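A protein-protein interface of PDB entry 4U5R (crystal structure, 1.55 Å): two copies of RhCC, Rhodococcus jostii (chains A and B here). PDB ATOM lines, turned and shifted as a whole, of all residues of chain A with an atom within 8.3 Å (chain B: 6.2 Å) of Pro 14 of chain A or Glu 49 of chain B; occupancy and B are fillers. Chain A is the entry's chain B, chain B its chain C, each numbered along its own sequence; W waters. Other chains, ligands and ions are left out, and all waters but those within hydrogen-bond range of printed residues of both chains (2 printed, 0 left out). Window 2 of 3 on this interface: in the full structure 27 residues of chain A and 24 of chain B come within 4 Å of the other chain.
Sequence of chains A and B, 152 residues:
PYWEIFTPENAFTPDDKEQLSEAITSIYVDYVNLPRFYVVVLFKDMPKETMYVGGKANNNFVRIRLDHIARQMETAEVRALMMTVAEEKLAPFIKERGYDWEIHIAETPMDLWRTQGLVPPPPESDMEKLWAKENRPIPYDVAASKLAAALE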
ATOM      1  N   ASN A  10      16.532   0.400 -11.378  1.00  0.00           N
ATOM      2  CA  ASN A  10      17.708   1.272 -11.459  1.00  0.00           C
ATOM      3  C   ASN A  10      17.587   2.578 -10.665  1.00  0.00           C
ATOM      4  O   ASN A  10      18.375   3.508 -10.862  1.00  0.00           O
ATOM      5  CB  ASN A  10      18.037   1.569 -12.937  1.00  0.00           C
ATOM      6  CG  ASN A  10      18.103   0.304 -13.789  1.00  0.00           C
ATOM      7  OD1 ASN A  10      17.468   0.215 -14.841  1.00  0.00           O
ATOM      8  ND2 ASN A  10      18.863  -0.683 -13.334  1.00  0.00           N
ATOM      9  N   ALA A  11      16.640   2.642  -9.729  1.00  0.00           N
ATOM     10  CA  ALA A  11      16.493   3.826  -8.885  1.00  0.00           C
ATOM     11  C   ALA A  11      17.755   4.111  -8.072  1.00  0.00           C
ATOM     12  O   ALA A  11      18.146   5.272  -7.908  1.00  0.00           O
ATOM     13  CB  ALA A  11      15.296   3.670  -7.939  1.00  0.00           C
ATOM     14  N   PHE A  12      18.369   3.048  -7.547  1.00  0.00           N
ATOM     15  CA  PHE A  12      19.537   3.170  -6.680  1.00  0.00           C
ATOM     16  C   PHE A  12      20.805   2.590  -7.283  1.00  0.00           C
ATOM     17  O   PHE A  12      20.798   1.491  -7.845  1.00  0.00           O
ATOM     18  CB  PHE A  12      19.282   2.480  -5.340  1.00  0.00           C
ATOM     19  CG  PHE A  12      18.180   3.098  -4.531  1.00  0.00           C
ATOM     20  CD1 PHE A  12      17.965   4.465  -4.536  1.00  0.00           C
ATOM     21  CD2 PHE A  12      17.375   2.300  -3.732  1.00  0.00           C
ATOM     22  CE1 PHE A  12      16.958   5.021  -3.772  1.00  0.00           C
ATOM     23  CE2 PHE A  12      16.365   2.851  -2.966  1.00  0.00           C
ATOM     24  CZ  PHE A  12      16.149   4.209  -2.992  1.00  0.00           C
ATOM     25  N   THR A  13      21.899   3.328  -7.129  1.00  0.00           N
ATOM     26  CA  THR A  13      23.229   2.837  -7.491  1.00  0.00           C
ATOM     27  C   THR A  13      23.731   1.880  -6.422  1.00  0.00           C
ATOM     28  O   THR A  13      23.183   1.844  -5.321  1.00  0.00           O
ATOM     29  CB  THR A  13      24.243   3.987  -7.633  1.00  0.00           C
ATOM     30  OG1 THR A  13      24.413   4.623  -6.362  1.00  0.00           O
ATOM     31  CG2 THR A  13      23.777   5.008  -8.670  1.00  0.00           C
ATOM     32  N   PRO A  14      24.788   1.108  -6.726  1.00  0.00           N
ATOM     33  CA  PRO A  14      25.361   0.280  -5.656  1.00  0.00           C
ATOM     34  C   PRO A  14      25.788   1.113  -4.434  1.00  0.00           C
ATOM     35  O   PRO A  14      25.571   0.700  -3.285  1.00  0.00           O
ATOM     36  CB  PRO A  14      26.567  -0.377  -6.336  1.00  0.00           C
ATOM     37  CG  PRO A  14      26.193  -0.436  -7.769  1.00  0.00           C
ATOM     38  CD  PRO A  14      25.384   0.804  -8.040  1.00  0.00           C
ATOM     39  N   ASP A  15      26.368   2.288  -4.679  1.00  0.00           N
ATOM     40  CA  ASP A  15      26.723   3.194  -3.595  1.00  0.00           C
ATOM     41  C   ASP A  15      25.491   3.646  -2.801  1.00  0.00           C
ATOM     42  O   ASP A  15      25.541   3.682  -1.577  1.00  0.00           O
ATOM     43  CB  ASP A  15      27.488   4.404  -4.138  1.00  0.00           C
ATOM     44  CG  ASP A  15      28.910   4.052  -4.554  1.00  0.00           C
ATOM     45  OD1 ASP A  15      29.389   2.958  -4.180  1.00  0.00           O
ATOM     46  OD2 ASP A  15      29.551   4.870  -5.250  1.00  0.00           O
ATOM     47  N   ASP A  16      24.390   3.959  -3.493  1.00  0.00           N
ATOM     48  CA  ASP A  16      23.114   4.275  -2.828  1.00  0.00           C
ATOM     49  C   ASP A  16      22.663   3.158  -1.892  1.00  0.00           C
ATOM     50  O   ASP A  16      22.186   3.407  -0.791  1.00  0.00           O
ATOM     51  CB  ASP A  16      21.984   4.488  -3.842  1.00  0.00           C
ATOM     52  CG  ASP A  16      22.024   5.838  -4.543  1.00  0.00           C
ATOM     53  OD1 ASP A  16      22.709   6.786  -4.087  1.00  0.00           O
ATOM     54  OD2 ASP A  16      21.323   5.938  -5.572  1.00  0.00           O
ATOM     55  N   LYS A  17      22.780   1.923  -2.361  1.00  0.00           N
ATOM     56  CA  LYS A  17      22.272   0.796  -1.583  1.00  0.00           C
ATOM     57  C   LYS A  17      23.142   0.555  -0.349  1.00  0.00           C
ATOM     58  O   LYS A  17      22.643   0.218   0.730  1.00  0.00           O
ATOM     59  CB  LYS A  17      22.178  -0.449  -2.471  1.00  0.00           C
ATOM     60  CG  LYS A  17      21.046  -0.359  -3.481  1.00  0.00           C
ATOM     61  CD  LYS A  17      20.942  -1.569  -4.386  1.00  0.00           C
ATOM     62  CE  LYS A  17      21.825  -1.426  -5.618  1.00  0.00           C
ATOM     63  NZ  LYS A  17      21.542  -2.520  -6.585  1.00  0.00           N
ATOM     64  N   GLU A  18      24.446   0.752  -0.503  1.00  0.00           N
ATOM     65  CA  GLU A  18      25.361   0.690   0.628  1.00  0.00           C
ATOM     66  C   GLU A  18      25.032   1.761   1.672  1.00  0.00           C
ATOM     67  O   GLU A  18      24.878   1.461   2.862  1.00  0.00           O
ATOM     68  CB  GLU A  18      26.800   0.844   0.139  1.00  0.00           C
ATOM     69  CG  GLU A  18      27.842   0.590   1.203  1.00  0.00           C
ATOM     70  CD  GLU A  18      29.221   0.477   0.603  1.00  0.00           C
ATOM     71  OE1 GLU A  18      29.636   1.419  -0.105  1.00  0.00           O
ATOM     72  OE2 GLU A  18      29.881  -0.561   0.822  1.00  0.00           O
ATOM     73  N   GLN A  19      24.895   3.004   1.221  1.00  0.00           N
ATOM     74  CA  GLN A  19      24.578   4.114   2.111  1.00  0.00           C
ATOM     75  C   GLN A  19      23.237   3.946   2.820  1.00  0.00           C
ATOM     76  O   GLN A  19      23.154   4.162   4.028  1.00  0.00           O
ATOM     77  CB  GLN A  19      24.601   5.436   1.336  1.00  0.00           C
ATOM     78  CG  GLN A  19      26.001   5.804   0.837  1.00  0.00           C
ATOM     79  CD  GLN A  19      26.019   7.047  -0.039  1.00  0.00           C
ATOM     80  OE1 GLN A  19      25.132   7.895   0.042  1.00  0.00           O
ATOM     81  NE2 GLN A  19      27.040   7.158  -0.884  1.00  0.00           N
ATOM     82  N   LEU A  20      22.194   3.559   2.083  1.00  0.00           N
ATOM     83  CA  LEU A  20      20.876   3.381   2.692  1.00  0.00           C
ATOM     84  C   LEU A  20      20.825   2.168   3.639  1.00  0.00           C
ATOM     85  O   LEU A  20      20.254   2.269   4.731  1.00  0.00           O
ATOM     86  CB  LEU A  20      19.807   3.259   1.602  1.00  0.00           C
ATOM     87  CG  LEU A  20      18.377   2.984   2.075  1.00  0.00           C
ATOM     88  CD1 LEU A  20      17.922   3.933   3.182  1.00  0.00           C
ATOM     89  CD2 LEU A  20      17.439   3.050   0.877  1.00  0.00           C
ATOM     90  N   SER A  21      21.439   1.050   3.255  1.00  0.00           N
ATOM     91  CA  SER A  21      21.478  -0.115   4.147  1.00  0.00           C
ATOM     92  C   SER A  21      22.314   0.173   5.393  1.00  0.00           C
ATOM     93  O   SER A  21      22.012  -0.334   6.479  1.00  0.00           O
ATOM     94  CB  SER A  21      22.002  -1.361   3.420  1.00  0.00           C
ATOM     95  OG  SER A  21      23.333  -1.204   2.958  1.00  0.00           O
ATOM     96  N   VAL A  41      19.000  -6.212   4.249  1.00  0.00           N
ATOM     97  CA  VAL A  41      18.190  -5.378   3.367  1.00  0.00           C
ATOM     98  C   VAL A  41      18.245  -5.936   1.944  1.00  0.00           C
ATOM     99  O   VAL A  41      19.316  -6.032   1.312  1.00  0.00           O
ATOM    100  CB  VAL A  41      18.650  -3.902   3.361  1.00  0.00           C
ATOM    101  CG1 VAL A  41      17.731  -3.087   2.459  1.00  0.00           C
ATOM    102  CG2 VAL A  41      18.638  -3.308   4.755  1.00  0.00           C
ATOM    103  N   LEU A  42      17.085  -6.315   1.428  1.00  0.00           N
ATOM    104  CA  LEU A  42      17.013  -6.874   0.087  1.00  0.00           C
ATOM    105  C   LEU A  42      16.416  -5.835  -0.861  1.00  0.00           C
ATOM    106  O   LEU A  42      15.270  -5.415  -0.675  1.00  0.00           O
ATOM    107  CB  LEU A  42      16.176  -8.167   0.070  1.00  0.00           C
ATOM    108  CG  LEU A  42      16.515  -9.246   1.110  1.00  0.00           C
ATOM    109  CD1 LEU A  42      15.631 -10.473   0.922  1.00  0.00           C
ATOM    110  CD2 LEU A  42      17.989  -9.630   1.028  1.00  0.00           C
ATOM    111  N   PHE A  43      17.204  -5.406  -1.845  1.00  0.00           N
ATOM    112  CA  PHE A  43      16.720  -4.476  -2.864  1.00  0.00           C
ATOM    113  C   PHE A  43      16.143  -5.216  -4.057  1.00  0.00           C
ATOM    114  O   PHE A  43      16.791  -6.078  -4.652  1.00  0.00           O
ATOM    115  CB  PHE A  43      17.843  -3.543  -3.324  1.00  0.00           C
ATOM    116  CG  PHE A  43      18.270  -2.577  -2.277  1.00  0.00           C
ATOM    117  CD1 PHE A  43      17.573  -1.394  -2.095  1.00  0.00           C
ATOM    118  CD2 PHE A  43      19.344  -2.854  -1.455  1.00  0.00           C
ATOM    119  CE1 PHE A  43      17.932  -0.510  -1.107  1.00  0.00           C
ATOM    120  CE2 PHE A  43      19.725  -1.963  -0.470  1.00  0.00           C
ATOM    121  CZ  PHE A  43      19.020  -0.780  -0.305  1.00  0.00           C
ATOM    122  N   LYS A  44      14.913  -4.874  -4.411  1.00  0.00           N
ATOM    123  CA  LYS A  44      14.229  -5.585  -5.474  1.00  0.00           C
ATOM    124  C   LYS A  44      13.795  -4.579  -6.537  1.00  0.00           C
ATOM    125  O   LYS A  44      12.857  -3.803  -6.335  1.00  0.00           O
ATOM    126  CB  LYS A  44      13.047  -6.377  -4.888  1.00  0.00           C
ATOM    127  CG  LYS A  44      13.504  -7.479  -3.907  1.00  0.00           C
ATOM    128  CD  LYS A  44      12.359  -8.069  -3.093  1.00  0.00           C
ATOM    129  CE  LYS A  44      12.806  -9.254  -2.262  1.00  0.00           C
ATOM    130  NZ  LYS A  44      11.618 -10.007  -1.774  1.00  0.00           N
ATOM    131  N   ASP A  45      14.518  -4.575  -7.656  1.00  0.00           N
ATOM    132  CA  ASP A  45      14.190  -3.725  -8.785  1.00  0.00           C
ATOM    133  C   ASP A  45      12.929  -4.230  -9.477  1.00  0.00           C
ATOM    134  O   ASP A  45      12.839  -5.403  -9.854  1.00  0.00           O
ATOM    135  CB  ASP A  45      15.366  -3.671  -9.771  1.00  0.00           C
ATOM    136  CG  ASP A  45      16.289  -2.490  -9.517  1.00  0.00           C
ATOM    137  OD1 ASP A  45      16.044  -1.723  -8.565  1.00  0.00           O
ATOM    138  OD2 ASP A  45      17.269  -2.332 -10.271  1.00  0.00           O
ATOM    139  N   PRO B  47      20.615 -10.529  -8.108  1.00  0.00           N
ATOM    140  CA  PRO B  47      21.886 -10.069  -8.685  1.00  0.00           C
ATOM    141  C   PRO B  47      22.886  -9.533  -7.657  1.00  0.00           C
ATOM    142  O   PRO B  47      22.527  -9.231  -6.522  1.00  0.00           O
ATOM    143  CB  PRO B  47      21.454  -8.947  -9.638  1.00  0.00           C
ATOM    144  CG  PRO B  47      20.025  -9.229  -9.954  1.00  0.00           C
ATOM    145  CD  PRO B  47      19.456  -9.825  -8.683  1.00  0.00           C
ATOM    146  N   LYS B  48      24.149  -9.413  -8.062  1.00  0.00           N
ATOM    147  CA  LYS B  48      25.159  -8.830  -7.194  1.00  0.00           C
ATOM    148  C   LYS B  48      24.716  -7.428  -6.802  1.00  0.00           C
ATOM    149  O   LYS B  48      23.990  -6.773  -7.554  1.00  0.00           O
ATOM    150  CB  LYS B  48      26.528  -8.810  -7.882  1.00  0.00           C
ATOM    151  CG  LYS B  48      27.125 -10.205  -8.055  1.00  0.00           C
ATOM    152  CD  LYS B  48      28.506 -10.167  -8.701  1.00  0.00           C
ATOM    153  CE  LYS B  48      29.096 -11.568  -8.806  1.00  0.00           C
ATOM    154  NZ  LYS B  48      30.456 -11.575  -9.421  1.00  0.00           N
ATOM    155  N   GLU B  49      25.127  -7.005  -5.612  1.00  0.00           N
ATOM    156  CA  GLU B  49      24.790  -5.693  -5.071  1.00  0.00           C
ATOM    157  C   GLU B  49      23.278  -5.506  -4.880  1.00  0.00           C
ATOM    158  O   GLU B  49      22.753  -4.409  -5.103  1.00  0.00           O
ATOM    159  CB  GLU B  49      25.355  -4.571  -5.963  1.00  0.00           C
ATOM    160  CG  GLU B  49      26.842  -4.315  -5.770  1.00  0.00           C
ATOM    161  CD  GLU B  49      27.710  -5.460  -6.251  1.00  0.00           C
ATOM    162  OE1 GLU B  49      28.448  -6.038  -5.426  1.00  0.00           O
ATOM    163  OE2 GLU B  49      27.664  -5.778  -7.458  1.00  0.00           O
ATOM    164  N   THR B  50      22.573  -6.561  -4.461  1.00  0.00           N
ATOM    165  CA  THR B  50      21.163  -6.397  -4.046  1.00  0.00           C
ATOM    166  C   THR B  50      20.832  -6.931  -2.647  1.00  0.00           C
ATOM    167  O   THR B  50      19.802  -6.553  -2.083  1.00  0.00           O
ATOM    168  CB  THR B  50      20.177  -7.051  -5.053  1.00  0.00           C
ATOM    169  OG1 THR B  50      20.375  -8.472  -5.113  1.00  0.00           O
ATOM    170  CG2 THR B  50      20.353  -6.439  -6.452  1.00  0.00           C
ATOM    171  N   MET B  51      21.686  -7.786  -2.086  1.00  0.00           N
ATOM    172  CA  MET B  51      21.494  -8.283  -0.724  1.00  0.00           C
ATOM    173  C   MET B  51      22.524  -7.642   0.187  1.00  0.00           C
ATOM    174  O   MET B  51      23.732  -7.874   0.052  1.00  0.00           O
ATOM    175  CB  MET B  51      21.611  -9.818  -0.664  1.00  0.00           C
ATOM    176  CG  MET B  51      20.709 -10.541  -1.660  1.00  0.00           C
ATOM    177  SD  MET B  51      20.807 -12.348  -1.641  1.00  0.00           S
ATOM    178  CE  MET B  51      19.905 -12.745  -0.140  1.00  0.00           C
ATOM    179  N   TYR B  52      22.056  -6.813   1.106  1.00  0.00           N
ATOM    180  CA  TYR B  52      22.968  -6.105   1.990  1.00  0.00           C
ATOM    181  C   TYR B  52      22.856  -6.586   3.434  1.00  0.00           C
ATOM    182  O   TYR B  52      21.779  -6.558   4.047  1.00  0.00           O
ATOM    183  CB  TYR B  52      22.721  -4.593   1.882  1.00  0.00           C
ATOM    184  CG  TYR B  52      23.271  -4.039   0.585  1.00  0.00           C
ATOM    185  CD1 TYR B  52      22.619  -4.265  -0.623  1.00  0.00           C
ATOM    186  CD2 TYR B  52      24.451  -3.308   0.576  1.00  0.00           C
ATOM    187  CE1 TYR B  52      23.135  -3.784  -1.815  1.00  0.00           C
ATOM    188  CE2 TYR B  52      24.978  -2.822  -0.612  1.00  0.00           C
ATOM    189  CZ  TYR B  52      24.311  -3.058  -1.797  1.00  0.00           C
ATOM    190  OH  TYR B  52      24.821  -2.580  -2.984  1.00  0.00           O
ATOM    191  N   ALA B  57      27.172  -5.209   0.879  1.00  0.00           N
ATOM    192  CA  ALA B  57      26.669  -6.237  -0.019  1.00  0.00           C
ATOM    193  C   ALA B  57      27.290  -7.584   0.351  1.00  0.00           C
ATOM    194  O   ALA B  57      28.491  -7.675   0.619  1.00  0.00           O
ATOM    195  CB  ALA B  57      26.972  -5.881  -1.476  1.00  0.00           C
ATOM    196  N   ASN B  59      27.336 -11.012  -1.638  1.00  0.00           N
ATOM    197  CA  ASN B  59      26.980 -11.668  -2.879  1.00  0.00           C
ATOM    198  C   ASN B  59      27.121 -13.174  -2.775  1.00  0.00           C
ATOM    199  O   ASN B  59      26.988 -13.883  -3.770  1.00  0.00           O
ATOM    200  CB  ASN B  59      27.836 -11.112  -4.021  1.00  0.00           C
ATOM    201  CG  ASN B  59      27.621  -9.621  -4.220  1.00  0.00           C
ATOM    202  OD1 ASN B  59      26.531  -9.105  -3.975  1.00  0.00           O
ATOM    203  ND2 ASN B  59      28.665  -8.916  -4.646  1.00  0.00           N
HETATM  204  O   HOH W   1      27.551  -1.959  -2.859  1.00  0.00           O
HETATM  205  O   HOH W   2      28.575  -2.848  -0.314  1.00  0.00           O
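Water W1 lies within hydrogen-bond range of the side-chain hydroxyl of Tyr 52 of chain B (2.8 Å) and the backbone carbonyl oxygen of Pro 14 of chain A (3.3 Å).
Water W2 lies within hydrogen-bond range of OE2 of Glu 18 of chain A (2.9 Å) and N of Ala 57 of chain B (3.0 Å).
Of the 8 printed residues of chain B, 4 touch a printed residue of chain A.
Hydrophobic or aromatic side chains of chain B within 4 Å of the printed part of chain A: Met 51 and Tyr 52.
Along chain B the printed residues that touch a printed residue of chain A span positions 49 to 52.
Printed residues of chain A that touch a printed residue of chain B: Pro 14, Lys 17, Glu 18, Ser 21, Val 41, Leu 42 and Phe 43.
Hydrophobic or aromatic side chains of chain A that line the printed part of chain B: Pro 14, Leu 42 and Phe 43.
Among the printed residues, 13 pairs touch across the chains.
Among the printed residues, no Asp or Glu carboxylate lies within 4 Å of a Lys or Arg side-chain nitrogen of the other chain.
Printed residues of chain B within 4 Å of Pro 14 of chain A: Glu 49 (3.99 Å) and Tyr 52 (3.4 Å).
Of the printed residues of chain B, Lys 17 of chain A touches Glu 49 and Tyr 52.
Of the printed residues of chain B, Glu 18 of chain A touches Tyr 52.
Asp 45 of chain A touches none of the printed residues of chain B.
Printed residues of chain A within 4 Å of Glu 49 of chain B: Pro 14 (3.99 Å) and Lys 17 (2.7 Å).
Printed residues of chain A within 4 Å of Tyr 52 of chain B: Pro 14 (3.4 Å), Lys 17 (3.4 Å), Glu 18 (3.6 Å), Ser 21 (3.4 Å), Val 41 (2.8 Å) and Phe 43 (3.7 Å).
No position is printed for both chains.
Of the 13 pairs that touch across the chains among the printed residues, none has its exchanged pair printed and touching as well.
Pro 14 of chain A touches Glu 49 of chain B.
Tyr 52 of chain B touches Lys 17 of chain A (OH to CB, 3.4 Å).
Glu 18 of chain A touches Tyr 52 of chain B (N to CE2, 3.6 Å).
Ser 21 of chain A touches Tyr 52 of chain B (OG to CD2, 3.4 Å).
Met 51 of chain B touches Val 41 of chain A.
O of Thr 50 of chain B touches CA of Leu 42 of chain A, at 3.5 Å.
Met 51 of chain B touches Leu 42 of chain A (CE to CD2, 3.8 Å).
Tyr 52 of chain B touches Phe 43 of chain A (CD1 to CD2, 3.7 Å).
The side-chain hydroxyl (OH) of Tyr 52 of chain B lies within hydrogen-bond range of the backbone carbonyl oxygen (O) of Pro 14 of chain A (3.4 Å).
The backbone carbonyl oxygen of Glu 49 of chain B lies within hydrogen-bond range of the side-chain amino group of Lys 17 of chain A, 2.7 Å away.
The backbone carbonyl oxygen (O) of Tyr 52 of chain B sits at hydrogen-bond distance from the backbone NH (N) of Val 41 of chain A (2.8 Å).
N of Phe 43 of chain A sits at hydrogen-bond distance from O of Thr 50 of chain B, at 2.8 Å.
O of Val 41 of chain A lies close to O of Thr 50 of chain B.
The backbone carbonyl oxygen (O) of Lys 17 of chain A is in hydrogen-bond range of the side-chain hydroxyl (OG) of Ser 21 of chain A, at 2.7 Å.
OG of Ser 21 of chain A is in hydrogen-bond range of O of Glu 18 of chain A (3.1 Å).
O of Pro 47 of chain B lies within hydrogen-bond range of OG1 of Thr 50 of chain B.
The side-chain hydroxyl of Tyr 52 of chain B lies close to the backbone carbonyl oxygen of Glu 49 of chain B.
ND2 of Asn 59 of chain B sits at hydrogen-bond distance from OE1 of Glu 49 of chain B (3.0 Å).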
